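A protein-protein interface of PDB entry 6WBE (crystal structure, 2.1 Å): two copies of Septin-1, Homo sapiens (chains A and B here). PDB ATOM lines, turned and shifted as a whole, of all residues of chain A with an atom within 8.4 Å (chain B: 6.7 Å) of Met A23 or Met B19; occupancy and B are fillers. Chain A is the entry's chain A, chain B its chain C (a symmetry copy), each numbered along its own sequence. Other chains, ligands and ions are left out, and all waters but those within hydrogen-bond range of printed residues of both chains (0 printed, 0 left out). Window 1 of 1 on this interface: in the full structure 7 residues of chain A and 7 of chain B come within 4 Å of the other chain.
Met A19 touches its own counterpart, Met B19.
Met A19 touches Met B23, and with the chains exchanged Met A23 touches Met B19.
Leu A20 touches its own counterpart, Leu B20.
Met A23 touches Leu B20, but with the chains exchanged Leu A20 does not touch Met B23 (4.1 Å).
The backbone carbonyl oxygen (O) of Leu B20 lies close to the side-chain amide oxygen (OE1) of Gln B24 (3.3 Å).
Among the printed residues, pairs that only touch across the chains: Met A27 with Met B16, Met A23 with Met B16, Leu A20 with Leu B20, Met A19 with Met B23, Met A16 with Met B23, Met A23 with Leu B20 and Met A19 with Met B19.
Of the 13 printed residues of chain B, 4 touch a printed residue of chain A.
Hydrophobic or aromatic side chains of chain B that line the printed part of chain A: Met B16, Met B19, Leu B20 and Met B23.
Along chain B the printed residues that touch a printed residue of chain A span positions 16 to 23.
Of the 14 printed residues of chain A, 5 touch a printed residue of chain B.
Printed residues of chain A that touch a printed residue of chain B: Met A16, Met A19, Leu A20, Met A23 and Met A27.
Hydrophobic or aromatic side chains of chain A that line the printed part of chain B: Met A16, Met A19, Leu A20, Met A23 and Met A27.
The side-chain sulfur (SD) of Met B19 sits close to the side-chain sulfur (SD) of Met A23, at 3.7 Å.
Met A23 touches three residues of chain B.
Printed residues of chain B within 4 Å of Met A27: Met B16 (3.5 Å).
Arg B15 touches none of the printed residues of chain A.
Printed residues of chain A within 4 Å of Met B16: Met A23 and Met A27.
Glu B21 touches none of the printed residues of chain A.
The nearest residue of chain A that does not touch Met B19 is Gln A26 (6.4 Å).
The nearest printed residue of chain A that does not touch Met B23 is Leu A20 (4.1 Å).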
ATOM      1  N   MET A  16      10.233  25.048  -0.351  1.00  0.00           N
ATOM      2  CA  MET A  16      10.515  25.553   0.993  1.00  0.00           C
ATOM      3  C   MET A  16       9.237  25.629   1.834  1.00  0.00           C
ATOM      4  O   MET A  16       9.250  25.250   3.010  1.00  0.00           O
ATOM      5  CB  MET A  16      11.233  26.918   0.918  1.00  0.00           C
ATOM      6  CG  MET A  16      12.646  26.852   0.284  1.00  0.00           C
ATOM      7  SD  MET A  16      13.483  28.452  -0.002  1.00  0.00           S
ATOM      8  CE  MET A  16      12.171  29.556   0.304  1.00  0.00           C
ATOM      9  N   GLN A  17       8.110  26.066   1.253  1.00  0.00           N
ATOM     10  CA  GLN A  17       6.882  26.099   2.041  1.00  0.00           C
ATOM     11  C   GLN A  17       6.529  24.710   2.551  1.00  0.00           C
ATOM     12  O   GLN A  17       6.152  24.550   3.711  1.00  0.00           O
ATOM     13  CB  GLN A  17       5.703  26.709   1.270  1.00  0.00           C
ATOM     14  CG  GLN A  17       5.772  28.266   1.162  1.00  0.00           C
ATOM     15  CD  GLN A  17       4.641  28.942   0.292  1.00  0.00           C
ATOM     16  OE1 GLN A  17       4.556  30.185   0.222  1.00  0.00           O
ATOM     17  NE2 GLN A  17       3.773  28.131  -0.331  1.00  0.00           N
ATOM     18  N   GLU A  18       6.656  23.699   1.698  1.00  0.00           N
ATOM     19  CA  GLU A  18       6.352  22.336   2.099  1.00  0.00           C
ATOM     20  C   GLU A  18       7.265  21.856   3.225  1.00  0.00           C
ATOM     21  O   GLU A  18       6.823  21.140   4.131  1.00  0.00           O
ATOM     22  CB  GLU A  18       6.479  21.455   0.873  1.00  0.00           C
ATOM     23  CG  GLU A  18       5.306  21.684  -0.056  1.00  0.00           C
ATOM     24  CD  GLU A  18       3.990  21.572   0.677  1.00  0.00           C
ATOM     25  OE1 GLU A  18       3.396  22.616   1.019  1.00  0.00           O
ATOM     26  OE2 GLU A  18       3.559  20.437   0.911  1.00  0.00           O
ATOM     27  N   MET A  19       8.540  22.236   3.181  1.00  0.00           N
ATOM     28  CA  MET A  19       9.478  21.865   4.229  1.00  0.00           C
ATOM     29  C   MET A  19       9.074  22.490   5.542  1.00  0.00           C
ATOM     30  O   MET A  19       8.992  21.803   6.568  1.00  0.00           O
ATOM     31  CB  MET A  19      10.881  22.339   3.856  1.00  0.00           C
ATOM     32  CG  MET A  19      11.513  21.633   2.672  1.00  0.00           C
ATOM     33  SD  MET A  19      13.163  22.243   2.206  1.00  0.00           S
ATOM     34  CE  MET A  19      14.167  21.666   3.563  1.00  0.00           C
ATOM     35  N   LEU A  20       8.767  23.799   5.514  1.00  0.00           N
ATOM     36  CA  LEU A  20       8.291  24.473   6.718  1.00  0.00           C
ATOM     37  C   LEU A  20       7.052  23.792   7.253  1.00  0.00           C
ATOM     38  O   LEU A  20       6.902  23.608   8.469  1.00  0.00           O
ATOM     39  CB  LEU A  20       7.956  25.935   6.433  1.00  0.00           C
ATOM     40  CG  LEU A  20       9.088  26.893   6.131  1.00  0.00           C
ATOM     41  CD1 LEU A  20       8.540  28.261   5.764  1.00  0.00           C
ATOM     42  CD2 LEU A  20       9.996  26.976   7.311  1.00  0.00           C
ATOM     43  N   GLU A  21       6.164  23.392   6.351  1.00  0.00           N
ATOM     44  CA  GLU A  21       4.954  22.739   6.788  1.00  0.00           C
ATOM     45  C   GLU A  21       5.294  21.426   7.478  1.00  0.00           C
ATOM     46  O   GLU A  21       4.835  21.184   8.586  1.00  0.00           O
ATOM     47  CB  GLU A  21       4.045  22.525   5.577  1.00  0.00           C
ATOM     48  CG  GLU A  21       2.630  21.980   5.830  1.00  0.00           C
ATOM     49  CD  GLU A  21       1.834  21.729   4.517  1.00  0.00           C
ATOM     50  OE1 GLU A  21       2.279  22.210   3.448  1.00  0.00           O
ATOM     51  OE2 GLU A  21       0.760  21.062   4.544  1.00  0.00           O
ATOM     52  N   LYS A  22       6.191  20.637   6.891  1.00  0.00           N
ATOM     53  CA  LYS A  22       6.608  19.375   7.485  1.00  0.00           C
ATOM     54  C   LYS A  22       7.344  19.597   8.795  1.00  0.00           C
ATOM     55  O   LYS A  22       7.231  18.791   9.716  1.00  0.00           O
ATOM     56  CB  LYS A  22       7.479  18.585   6.503  1.00  0.00           C
ATOM     57  N   MET A  23       8.125  20.669   8.889  1.00  0.00           N
ATOM     58  CA  MET A  23       8.766  20.970  10.168  1.00  0.00           C
ATOM     59  C   MET A  23       7.750  21.322  11.239  1.00  0.00           C
ATOM     60  O   MET A  23       7.880  20.882  12.383  1.00  0.00           O
ATOM     61  CB  MET A  23       9.763  22.112  10.001  1.00  0.00           C
ATOM     62  CG  MET A  23      10.968  21.725   9.190  1.00  0.00           C
ATOM     63  SD  MET A  23      11.996  23.158   8.822  1.00  0.00           S
ATOM     64  CE  MET A  23      11.893  23.949  10.394  1.00  0.00           C
ATOM     65  N   GLN A  24       6.754  22.150  10.917  1.00  0.00           N
ATOM     66  CA  GLN A  24       5.840  22.549  11.984  1.00  0.00           C
ATOM     67  C   GLN A  24       5.083  21.345  12.501  1.00  0.00           C
ATOM     68  O   GLN A  24       4.857  21.211  13.716  1.00  0.00           O
ATOM     69  CB  GLN A  24       4.883  23.637  11.508  1.00  0.00           C
ATOM     70  CG  GLN A  24       5.422  25.047  11.696  1.00  0.00           C
ATOM     71  CD  GLN A  24       4.668  26.047  10.857  1.00  0.00           C
ATOM     72  OE1 GLN A  24       3.508  25.824  10.485  1.00  0.00           O
ATOM     73  NE2 GLN A  24       5.328  27.143  10.516  1.00  0.00           N
ATOM     74  N   ALA A  25       4.718  20.436  11.587  1.00  0.00           N
ATOM     75  CA  ALA A  25       4.025  19.219  11.995  1.00  0.00           C
ATOM     76  C   ALA A  25       4.882  18.394  12.933  1.00  0.00           C
ATOM     77  O   ALA A  25       4.372  17.822  13.911  1.00  0.00           O
ATOM     78  CB  ALA A  25       3.646  18.383  10.775  1.00  0.00           C
ATOM     79  N   GLN A  26       6.190  18.339  12.675  1.00  0.00           N
ATOM     80  CA  GLN A  26       7.053  17.565  13.562  1.00  0.00           C
ATOM     81  C   GLN A  26       7.071  18.144  14.957  1.00  0.00           C
ATOM     82  O   GLN A  26       7.055  17.394  15.943  1.00  0.00           O
ATOM     83  CB  GLN A  26       8.477  17.519  13.043  1.00  0.00           C
ATOM     84  CG  GLN A  26       8.683  16.810  11.741  1.00  0.00           C
ATOM     85  CD  GLN A  26      10.129  16.368  11.621  1.00  0.00           C
ATOM     86  OE1 GLN A  26      10.803  16.116  12.647  1.00  0.00           O
ATOM     87  NE2 GLN A  26      10.629  16.291  10.386  1.00  0.00           N
ATOM     88  N   MET A  27       7.004  19.462  15.072  1.00  0.00           N
ATOM     89  CA  MET A  27       7.022  20.016  16.414  1.00  0.00           C
ATOM     90  C   MET A  27       5.661  19.932  17.109  1.00  0.00           C
ATOM     91  O   MET A  27       5.599  20.076  18.339  1.00  0.00           O
ATOM     92  CB  MET A  27       7.578  21.440  16.342  1.00  0.00           C
ATOM     93  CG  MET A  27       9.052  21.421  15.889  1.00  0.00           C
ATOM     94  SD  MET A  27       9.899  22.993  15.872  1.00  0.00           S
ATOM     95  CE  MET A  27       9.328  23.686  14.329  1.00  0.00           C
ATOM     96  N   GLN A  28       4.584  19.625  16.371  1.00  0.00           N
ATOM     97  CA  GLN A  28       3.315  19.234  16.979  1.00  0.00           C
ATOM     98  C   GLN A  28       3.354  17.772  17.397  1.00  0.00           C
ATOM     99  O   GLN A  28       3.647  17.439  18.553  1.00  0.00           O
ATOM    100  CB  GLN A  28       2.152  19.451  16.005  1.00  0.00           C
ATOM    101  N   GLN A  29       3.056  16.900  16.442  1.00  0.00           N
ATOM    102  CA  GLN A  29       3.072  15.463  16.653  1.00  0.00           C
ATOM    103  C   GLN A  29       4.440  14.881  16.348  1.00  0.00           C
ATOM    104  O   GLN A  29       4.719  14.535  15.203  1.00  0.00           O
ATOM    105  CB  GLN A  29       2.004  14.787  15.783  1.00  0.00           C
ATOM    106  N   LEU B  13      16.061  19.092  16.258  1.00  0.00           N
ATOM    107  CA  LEU B  13      15.990  20.553  16.144  1.00  0.00           C
ATOM    108  C   LEU B  13      17.170  21.115  15.345  1.00  0.00           C
ATOM    109  O   LEU B  13      17.021  22.091  14.592  1.00  0.00           O
ATOM    110  CB  LEU B  13      15.954  21.157  17.538  1.00  0.00           C
ATOM    111  CG  LEU B  13      14.748  20.674  18.353  1.00  0.00           C
ATOM    112  CD1 LEU B  13      14.858  21.318  19.726  1.00  0.00           C
ATOM    113  CD2 LEU B  13      13.394  20.982  17.691  1.00  0.00           C
ATOM    114  N   ARG B  14      18.360  20.515  15.501  1.00  0.00           N
ATOM    115  CA  ARG B  14      19.523  20.978  14.746  1.00  0.00           C
ATOM    116  C   ARG B  14      19.295  20.782  13.271  1.00  0.00           C
ATOM    117  O   ARG B  14      19.676  21.644  12.470  1.00  0.00           O
ATOM    118  CB  ARG B  14      20.779  20.214  15.131  1.00  0.00           C
ATOM    119  CG  ARG B  14      21.387  20.560  16.516  1.00  0.00           C
ATOM    120  CD  ARG B  14      22.685  19.774  16.747  1.00  0.00           C
ATOM    121  NE  ARG B  14      23.426  20.328  17.899  1.00  0.00           N
ATOM    122  CZ  ARG B  14      24.075  19.605  18.790  1.00  0.00           C
ATOM    123  NH1 ARG B  14      24.714  20.211  19.790  1.00  0.00           N
ATOM    124  NH2 ARG B  14      24.062  18.276  18.697  1.00  0.00           N
ATOM    125  N   ARG B  15      18.674  19.643  12.898  1.00  0.00           N
ATOM    126  CA  ARG B  15      18.392  19.364  11.498  1.00  0.00           C
ATOM    127  C   ARG B  15      17.387  20.365  10.964  1.00  0.00           C
ATOM    128  O   ARG B  15      17.519  20.846   9.836  1.00  0.00           O
ATOM    129  CB  ARG B  15      17.879  17.922  11.314  1.00  0.00           C
ATOM    130  CG  ARG B  15      18.933  16.825  11.587  1.00  0.00           C
ATOM    131  CD  ARG B  15      18.547  15.417  11.016  1.00  0.00           C
ATOM    132  NE  ARG B  15      17.552  14.617  11.754  1.00  0.00           N
ATOM    133  CZ  ARG B  15      17.847  13.658  12.646  1.00  0.00           C
ATOM    134  NH1 ARG B  15      19.114  13.355  12.911  1.00  0.00           N
ATOM    135  NH2 ARG B  15      16.878  12.985  13.265  1.00  0.00           N
ATOM    136  N   MET B  16      16.402  20.738  11.779  1.00  0.00           N
ATOM    137  CA  MET B  16      15.482  21.765  11.309  1.00  0.00           C
ATOM    138  C   MET B  16      16.158  23.114  11.234  1.00  0.00           C
ATOM    139  O   MET B  16      15.966  23.842  10.259  1.00  0.00           O
ATOM    140  CB  MET B  16      14.243  21.807  12.175  1.00  0.00           C
ATOM    141  CG  MET B  16      13.442  20.538  11.921  1.00  0.00           C
ATOM    142  SD  MET B  16      11.968  20.432  12.871  1.00  0.00           S
ATOM    143  CE  MET B  16      12.511  21.195  14.327  1.00  0.00           C
ATOM    144  N   GLN B  17      16.968  23.451  12.239  1.00  0.00           N
ATOM    145  CA  GLN B  17      17.659  24.728  12.201  1.00  0.00           C
ATOM    146  C   GLN B  17      18.561  24.809  10.990  1.00  0.00           C
ATOM    147  O   GLN B  17      18.653  25.853  10.334  1.00  0.00           O
ATOM    148  CB  GLN B  17      18.463  24.942  13.473  1.00  0.00           C
ATOM    149  CG  GLN B  17      19.321  26.166  13.450  1.00  0.00           C
ATOM    150  CD  GLN B  17      18.526  27.476  13.426  1.00  0.00           C
ATOM    151  OE1 GLN B  17      17.296  27.513  13.650  1.00  0.00           O
ATOM    152  NE2 GLN B  17      19.249  28.574  13.125  1.00  0.00           N
ATOM    153  N   GLU B  18      19.280  23.730  10.717  1.00  0.00           N
ATOM    154  CA  GLU B  18      20.145  23.704   9.548  1.00  0.00           C
ATOM    155  C   GLU B  18      19.338  23.838   8.261  1.00  0.00           C
ATOM    156  O   GLU B  18      19.719  24.589   7.359  1.00  0.00           O
ATOM    157  CB  GLU B  18      20.969  22.417   9.567  1.00  0.00           C
ATOM    158  CG  GLU B  18      22.445  22.653   9.503  1.00  0.00           C
ATOM    159  CD  GLU B  18      23.254  21.400   9.789  1.00  0.00           C
ATOM    160  OE1 GLU B  18      22.717  20.456  10.439  1.00  0.00           O
ATOM    161  OE2 GLU B  18      24.437  21.373   9.360  1.00  0.00           O
ATOM    162  N   MET B  19      18.190  23.181   8.153  1.00  0.00           N
ATOM    163  CA  MET B  19      17.442  23.400   6.906  1.00  0.00           C
ATOM    164  C   MET B  19      16.909  24.834   6.815  1.00  0.00           C
ATOM    165  O   MET B  19      16.900  25.430   5.736  1.00  0.00           O
ATOM    166  CB  MET B  19      16.354  22.348   6.686  1.00  0.00           C
ATOM    167  CG  MET B  19      15.407  22.041   7.797  1.00  0.00           C
ATOM    168  SD  MET B  19      14.289  20.702   7.256  1.00  0.00           S
ATOM    169  CE  MET B  19      15.386  19.274   7.257  1.00  0.00           C
ATOM    170  N   LEU B  20      16.483  25.413   7.932  1.00  0.00           N
ATOM    171  CA  LEU B  20      16.094  26.826   7.949  1.00  0.00           C
ATOM    172  C   LEU B  20      17.218  27.745   7.449  1.00  0.00           C
ATOM    173  O   LEU B  20      16.969  28.715   6.731  1.00  0.00           O
ATOM    174  CB  LEU B  20      15.742  27.188   9.383  1.00  0.00           C
ATOM    175  CG  LEU B  20      14.415  27.863   9.623  1.00  0.00           C
ATOM    176  CD1 LEU B  20      13.291  27.154   8.886  1.00  0.00           C
ATOM    177  CD2 LEU B  20      14.180  27.902  11.107  1.00  0.00           C
ATOM    178  N   GLU B  21      18.458  27.469   7.845  1.00  0.00           N
ATOM    179  CA  GLU B  21      19.577  28.296   7.415  1.00  0.00           C
ATOM    180  C   GLU B  21      19.811  28.187   5.922  1.00  0.00           C
ATOM    181  O   GLU B  21      20.106  29.190   5.274  1.00  0.00           O
ATOM    182  CB  GLU B  21      20.831  27.903   8.198  1.00  0.00           C
ATOM    183  CG  GLU B  21      20.659  28.269   9.654  1.00  0.00           C
ATOM    184  CD  GLU B  21      21.695  27.657  10.612  1.00  0.00           C
ATOM    185  OE1 GLU B  21      22.459  26.706  10.283  1.00  0.00           O
ATOM    186  OE2 GLU B  21      21.766  28.220  11.713  1.00  0.00           O
ATOM    187  N   LYS B  22      19.680  26.987   5.358  1.00  0.00           N
ATOM    188  CA  LYS B  22      19.814  26.816   3.918  1.00  0.00           C
ATOM    189  C   LYS B  22      18.732  27.579   3.157  1.00  0.00           C
ATOM    190  O   LYS B  22      18.986  28.104   2.075  1.00  0.00           O
ATOM    191  CB  LYS B  22      19.768  25.329   3.577  1.00  0.00           C
ATOM    192  N   MET B  23      17.510  27.634   3.685  1.00  0.00           N
ATOM    193  CA  MET B  23      16.476  28.414   3.015  1.00  0.00           C
ATOM    194  C   MET B  23      16.821  29.891   3.006  1.00  0.00           C
ATOM    195  O   MET B  23      16.771  30.541   1.962  1.00  0.00           O
ATOM    196  CB  MET B  23      15.123  28.212   3.684  1.00  0.00           C
ATOM    197  CG  MET B  23      14.549  26.849   3.546  1.00  0.00           C
ATOM    198  SD  MET B  23      12.979  26.863   4.415  1.00  0.00           S
ATOM    199  CE  MET B  23      12.884  25.194   5.040  1.00  0.00           C
ATOM    200  N   GLN B  24      17.207  30.439   4.159  1.00  0.00           N
ATOM    201  CA  GLN B  24      17.514  31.866   4.175  1.00  0.00           C
ATOM    202  C   GLN B  24      18.712  32.179   3.285  1.00  0.00           C
ATOM    203  O   GLN B  24      18.683  33.146   2.518  1.00  0.00           O
ATOM    204  CB  GLN B  24      17.745  32.343   5.610  1.00  0.00           C
ATOM    205  CG  GLN B  24      16.464  32.607   6.396  1.00  0.00           C
ATOM    206  CD  GLN B  24      16.426  31.962   7.802  1.00  0.00           C
ATOM    207  OE1 GLN B  24      17.445  31.554   8.378  1.00  0.00           O
ATOM    208  NE2 GLN B  24      15.227  31.877   8.351  1.00  0.00           N
ATOM    209  N   GLN B  26      19.655  30.465   0.682  1.00  0.00           N
ATOM    210  CA  GLN B  26      19.212  30.204  -0.673  1.00  0.00           C
ATOM    211  C   GLN B  26      18.413  31.367  -1.210  1.00  0.00           C
ATOM    212  O   GLN B  26      18.446  31.638  -2.411  1.00  0.00           O
ATOM    213  CB  GLN B  26      18.374  28.927  -0.690  1.00  0.00           C
ATOM    214  CG  GLN B  26      18.275  28.187  -2.003  1.00  0.00           C
ATOM    215  CD  GLN B  26      17.717  26.778  -1.804  1.00  0.00           C
ATOM    216  OE1 GLN B  26      17.369  26.393  -0.688  1.00  0.00           O
ATOM    217  NE2 GLN B  26      17.581  26.027  -2.897  1.00  0.00           N
